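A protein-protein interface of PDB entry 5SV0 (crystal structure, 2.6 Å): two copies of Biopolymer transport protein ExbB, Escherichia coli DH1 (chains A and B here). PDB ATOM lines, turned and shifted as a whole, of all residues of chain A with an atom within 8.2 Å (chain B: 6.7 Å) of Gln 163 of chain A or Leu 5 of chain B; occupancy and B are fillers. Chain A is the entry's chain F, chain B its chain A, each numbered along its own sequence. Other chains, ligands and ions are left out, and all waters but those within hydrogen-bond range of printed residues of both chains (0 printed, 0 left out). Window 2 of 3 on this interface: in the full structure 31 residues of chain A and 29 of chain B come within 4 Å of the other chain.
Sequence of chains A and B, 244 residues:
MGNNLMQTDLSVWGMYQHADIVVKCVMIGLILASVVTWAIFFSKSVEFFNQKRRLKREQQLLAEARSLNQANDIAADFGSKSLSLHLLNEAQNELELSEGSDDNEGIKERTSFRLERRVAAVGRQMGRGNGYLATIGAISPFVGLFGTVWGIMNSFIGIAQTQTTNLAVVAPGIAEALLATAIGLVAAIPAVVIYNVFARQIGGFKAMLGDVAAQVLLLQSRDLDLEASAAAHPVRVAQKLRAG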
ATOM      1  N   ILE A 157      -2.423  29.468 -18.130  1.00  0.00           N
ATOM      2  CA  ILE A 157      -2.055  30.316 -19.259  1.00  0.00           C
ATOM      3  C   ILE A 157      -0.625  30.021 -19.671  1.00  0.00           C
ATOM      4  O   ILE A 157      -0.286  30.058 -20.852  1.00  0.00           O
ATOM      5  CB  ILE A 157      -2.232  31.802 -18.893  1.00  0.00           C
ATOM      6  CG1 ILE A 157      -3.682  32.130 -18.559  1.00  0.00           C
ATOM      7  CG2 ILE A 157      -1.793  32.678 -20.026  1.00  0.00           C
ATOM      8  CD1 ILE A 157      -3.883  33.573 -18.060  1.00  0.00           C
ATOM      9  N   GLY A 158       0.221  29.682 -18.701  1.00  0.00           N
ATOM     10  CA  GLY A 158       1.616  29.394 -18.982  1.00  0.00           C
ATOM     11  C   GLY A 158       1.838  28.179 -19.857  1.00  0.00           C
ATOM     12  O   GLY A 158       2.714  28.191 -20.727  1.00  0.00           O
ATOM     13  N   ILE A 159       1.096  27.096 -19.608  1.00  0.00           N
ATOM     14  CA  ILE A 159       1.342  25.891 -20.404  1.00  0.00           C
ATOM     15  C   ILE A 159       1.157  26.153 -21.892  1.00  0.00           C
ATOM     16  O   ILE A 159       1.864  25.567 -22.727  1.00  0.00           O
ATOM     17  CB  ILE A 159       0.438  24.732 -19.954  1.00  0.00           C
ATOM     18  CG1 ILE A 159      -0.479  24.308 -21.098  1.00  0.00           C
ATOM     19  CG2 ILE A 159      -0.357  25.115 -18.756  1.00  0.00           C
ATOM     20  CD1 ILE A 159      -1.567  23.433 -20.678  1.00  0.00           C
ATOM     21  N   ALA A 160       0.238  27.039 -22.252  1.00  0.00           N
ATOM     22  CA  ALA A 160      -0.004  27.323 -23.649  1.00  0.00           C
ATOM     23  C   ALA A 160      -0.013  28.822 -23.811  1.00  0.00           C
ATOM     24  O   ALA A 160      -0.946  29.449 -23.340  1.00  0.00           O
ATOM     25  CB  ALA A 160      -1.314  26.719 -24.084  1.00  0.00           C
ATOM     26  N   GLN A 161       0.943  29.403 -24.538  1.00  0.00           N
ATOM     27  CA  GLN A 161       1.779  28.702 -25.506  1.00  0.00           C
ATOM     28  C   GLN A 161       3.008  28.060 -24.884  1.00  0.00           C
ATOM     29  O   GLN A 161       3.175  28.076 -23.675  1.00  0.00           O
ATOM     30  CB  GLN A 161       2.202  29.666 -26.626  1.00  0.00           C
ATOM     31  N   THR A 162       3.874  27.556 -25.762  1.00  0.00           N
ATOM     32  CA  THR A 162       4.874  26.509 -25.552  1.00  0.00           C
ATOM     33  C   THR A 162       4.172  25.157 -25.555  1.00  0.00           C
ATOM     34  O   THR A 162       4.791  24.129 -25.846  1.00  0.00           O
ATOM     35  CB  THR A 162       5.669  26.689 -24.247  1.00  0.00           C
ATOM     36  OG1 THR A 162       4.822  26.428 -23.118  1.00  0.00           O
ATOM     37  CG2 THR A 162       6.260  28.099 -24.149  1.00  0.00           C
ATOM     38  N   GLN A 163       2.868  25.173 -25.267  1.00  0.00           N
ATOM     39  CA  GLN A 163       1.918  24.111 -25.622  1.00  0.00           C
ATOM     40  C   GLN A 163       2.384  22.711 -25.217  1.00  0.00           C
ATOM     41  O   GLN A 163       1.985  21.717 -25.834  1.00  0.00           O
ATOM     42  CB  GLN A 163       1.578  24.154 -27.112  1.00  0.00           C
ATOM     43  CG  GLN A 163       0.599  25.264 -27.472  1.00  0.00           C
ATOM     44  CD  GLN A 163       1.052  26.096 -28.657  1.00  0.00           C
ATOM     45  OE1 GLN A 163       2.149  26.655 -28.666  1.00  0.00           O
ATOM     46  NE2 GLN A 163       0.204  26.183 -29.664  1.00  0.00           N
ATOM     47  N   THR A 164       3.193  22.604 -24.165  1.00  0.00           N
ATOM     48  CA  THR A 164       3.651  21.314 -23.664  1.00  0.00           C
ATOM     49  C   THR A 164       3.145  21.145 -22.237  1.00  0.00           C
ATOM     50  O   THR A 164       2.769  22.118 -21.578  1.00  0.00           O
ATOM     51  CB  THR A 164       5.190  21.177 -23.728  1.00  0.00           C
ATOM     52  OG1 THR A 164       5.813  22.320 -23.134  1.00  0.00           O
ATOM     53  CG2 THR A 164       5.673  21.034 -25.181  1.00  0.00           C
ATOM     54  N   THR A 165       3.087  19.891 -21.777  1.00  0.00           N
ATOM     55  CA  THR A 165       2.617  19.629 -20.420  1.00  0.00           C
ATOM     56  C   THR A 165       3.778  19.660 -19.430  1.00  0.00           C
ATOM     57  O   THR A 165       3.973  20.666 -18.742  1.00  0.00           O
ATOM     58  CB  THR A 165       1.889  18.276 -20.354  1.00  0.00           C
ATOM     59  OG1 THR A 165       0.698  18.329 -21.149  1.00  0.00           O
ATOM     60  CG2 THR A 165       1.511  17.917 -18.921  1.00  0.00           C
ATOM     61  N   ASN A 166       4.570  18.583 -19.380  1.00  0.00           N
ATOM     62  CA  ASN A 166       5.702  18.473 -18.465  1.00  0.00           C
ATOM     63  C   ASN A 166       5.326  18.973 -17.071  1.00  0.00           C
ATOM     64  O   ASN A 166       4.209  18.745 -16.592  1.00  0.00           O
ATOM     65  CB  ASN A 166       6.912  19.242 -19.005  1.00  0.00           C
ATOM     66  N   VAL A 169       7.141  24.481 -16.189  1.00  0.00           N
ATOM     67  CA  VAL A 169       6.436  25.753 -16.360  1.00  0.00           C
ATOM     68  C   VAL A 169       5.107  25.765 -15.607  1.00  0.00           C
ATOM     69  O   VAL A 169       4.554  26.845 -15.348  1.00  0.00           O
ATOM     70  CB  VAL A 169       6.216  26.098 -17.843  1.00  0.00           C
ATOM     71  CG1 VAL A 169       5.814  27.571 -17.989  1.00  0.00           C
ATOM     72  CG2 VAL A 169       7.482  25.809 -18.644  1.00  0.00           C
ATOM     73  N   ASN B   3       7.333  18.768 -33.418  1.00  0.00           N
ATOM     74  CA  ASN B   3       8.377  19.785 -33.358  1.00  0.00           C
ATOM     75  C   ASN B   3       7.723  21.139 -33.590  1.00  0.00           C
ATOM     76  O   ASN B   3       6.699  21.248 -34.274  1.00  0.00           O
ATOM     77  CB  ASN B   3       9.476  19.541 -34.403  1.00  0.00           C
ATOM     78  CG  ASN B   3      10.569  20.603 -34.388  1.00  0.00           C
ATOM     79  OD1 ASN B   3      10.637  21.441 -33.484  1.00  0.00           O
ATOM     80  ND2 ASN B   3      11.436  20.568 -35.399  1.00  0.00           N
ATOM     81  N   ASN B   4       8.386  22.178 -33.078  1.00  0.00           N
ATOM     82  CA  ASN B   4       7.909  23.558 -33.120  1.00  0.00           C
ATOM     83  C   ASN B   4       6.437  23.684 -32.751  1.00  0.00           C
ATOM     84  O   ASN B   4       6.023  23.288 -31.658  1.00  0.00           O
ATOM     85  CB  ASN B   4       8.154  24.176 -34.495  1.00  0.00           C
ATOM     86  CG  ASN B   4       9.311  25.150 -34.487  1.00  0.00           C
ATOM     87  OD1 ASN B   4       9.928  25.382 -33.446  1.00  0.00           O
ATOM     88  ND2 ASN B   4       9.620  25.721 -35.648  1.00  0.00           N
ATOM     89  N   LEU B   5       5.652  24.238 -33.668  1.00  0.00           N
ATOM     90  CA  LEU B   5       4.237  24.498 -33.494  1.00  0.00           C
ATOM     91  C   LEU B   5       3.718  25.099 -34.783  1.00  0.00           C
ATOM     92  O   LEU B   5       4.485  25.592 -35.616  1.00  0.00           O
ATOM     93  CB  LEU B   5       3.967  25.480 -32.353  1.00  0.00           C
ATOM     94  CG  LEU B   5       3.317  24.944 -31.089  1.00  0.00           C
ATOM     95  CD1 LEU B   5       2.773  23.556 -31.355  1.00  0.00           C
ATOM     96  CD2 LEU B   5       4.318  24.961 -29.936  1.00  0.00           C
ATOM     97  N   MET B   6       2.407  25.023 -34.952  1.00  0.00           N
ATOM     98  CA  MET B   6       1.655  26.094 -35.579  1.00  0.00           C
ATOM     99  C   MET B   6       0.482  26.346 -34.651  1.00  0.00           C
ATOM    100  O   MET B   6      -0.433  25.519 -34.577  1.00  0.00           O
ATOM    101  CB  MET B   6       1.198  25.722 -36.991  1.00  0.00           C
ATOM    102  N   GLN B   7       0.541  27.460 -33.921  1.00  0.00           N
ATOM    103  CA  GLN B   7      -0.547  27.979 -33.098  1.00  0.00           C
ATOM    104  C   GLN B   7      -0.010  29.115 -32.245  1.00  0.00           C
ATOM    105  O   GLN B   7       1.189  29.411 -32.283  1.00  0.00           O
ATOM    106  CB  GLN B   7      -1.176  26.905 -32.207  1.00  0.00           C
ATOM    107  N   THR B   8      -0.896  29.768 -31.500  1.00  0.00           N
ATOM    108  CA  THR B   8      -0.571  30.637 -30.366  1.00  0.00           C
ATOM    109  C   THR B   8      -1.884  30.866 -29.620  1.00  0.00           C
ATOM    110  O   THR B   8      -2.907  30.246 -29.934  1.00  0.00           O
ATOM    111  CB  THR B   8       0.098  31.952 -30.793  1.00  0.00           C
ATOM    112  OG1 THR B   8       0.908  31.749 -31.959  1.00  0.00           O
ATOM    113  CG2 THR B   8       1.005  32.475 -29.681  1.00  0.00           C
ATOM    114  N   ASP B   9      -1.856  31.746 -28.625  1.00  0.00           N
ATOM    115  CA  ASP B   9      -2.997  32.107 -27.793  1.00  0.00           C
ATOM    116  C   ASP B   9      -3.352  33.579 -28.024  1.00  0.00           C
ATOM    117  O   ASP B   9      -2.861  34.212 -28.966  1.00  0.00           O
ATOM    118  CB  ASP B   9      -2.697  31.809 -26.322  1.00  0.00           C
ATOM    119  N   ASN B 166      -3.027  15.654 -24.495  1.00  0.00           N
ATOM    120  CA  ASN B 166      -2.236  16.876 -24.381  1.00  0.00           C
ATOM    121  C   ASN B 166      -2.945  17.861 -23.468  1.00  0.00           C
ATOM    122  O   ASN B 166      -3.708  17.452 -22.592  1.00  0.00           O
ATOM    123  CB  ASN B 166      -1.988  17.512 -25.745  1.00  0.00           C
ATOM    124  CG  ASN B 166      -0.654  18.221 -25.806  1.00  0.00           C
ATOM    125  OD1 ASN B 166      -0.538  19.389 -25.431  1.00  0.00           O
ATOM    126  ND2 ASN B 166       0.375  17.501 -26.246  1.00  0.00           N
ATOM    127  N   LEU B 167      -2.736  19.159 -23.656  1.00  0.00           N
ATOM    128  CA  LEU B 167      -3.649  20.057 -22.972  1.00  0.00           C
ATOM    129  C   LEU B 167      -4.069  21.178 -23.902  1.00  0.00           C
ATOM    130  O   LEU B 167      -4.998  21.004 -24.691  1.00  0.00           O
ATOM    131  CB  LEU B 167      -3.002  20.602 -21.710  1.00  0.00           C
ATOM    132  N   ALA B 168      -3.388  22.327 -23.821  1.00  0.00           N
ATOM    133  CA  ALA B 168      -3.205  23.323 -24.880  1.00  0.00           C
ATOM    134  C   ALA B 168      -4.486  23.711 -25.614  1.00  0.00           C
ATOM    135  O   ALA B 168      -4.591  24.805 -26.180  1.00  0.00           O
ATOM    136  CB  ALA B 168      -2.171  22.821 -25.883  1.00  0.00           C
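The backbone carbonyl oxygen (O) of Ile 159 of chain A lies within hydrogen-bond range of the side-chain hydroxyl (OG1) of Thr 162 of chain A, 3.1 Å away.
Of the printed residues of chain B, Ala 160 of chain A touches Ala 168. Thr 164 of chain A touches none of the printed residues of chain B. Of chain A, only Gln 163 comes within 4 Å of Leu 5 of chain B. Of the printed residues of chain A, Gln 7 of chain B touches Gln 163. Of the printed residues of chain A, Asn 166 of chain B touches Gln 163 (3.5 Å). Printed residues of chain A within 4 Å of Leu 167 of chain B: Ile 159 (3.3 Å). The nearest residue of chain B that does not touch Gln 163 of chain A is Ala 168 of chain B (4.02 Å). The nearest residue of chain A that does not touch Leu 5 of chain B is Thr 162 of chain A (4.2 Å). The nearest printed residue of chain A that does not touch Leu 167 of chain B is Thr 165 of chain A (4.3 Å).
Of the 10 printed residues of chain B, 5 touch a printed residue of chain A.
Position printed for both chains: 166.
Among the printed residues, merely in contact across the chains: Ile 159 of chain A with Leu 167 of chain B (3.3 Å), Ile 159 of chain A with Ala 168 of chain B (3.8 Å), Ala 160 of chain A with Ala 168 of chain B (3.97 Å), Gln 163 of chain A with Leu 5 of chain B (3.0 Å) and Gln 163 of chain A with Gln 7 of chain B (3.0 Å).
OD1 of Asn 166 of chain B sits close to O of Gln 163 of chain A (3.5 Å).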
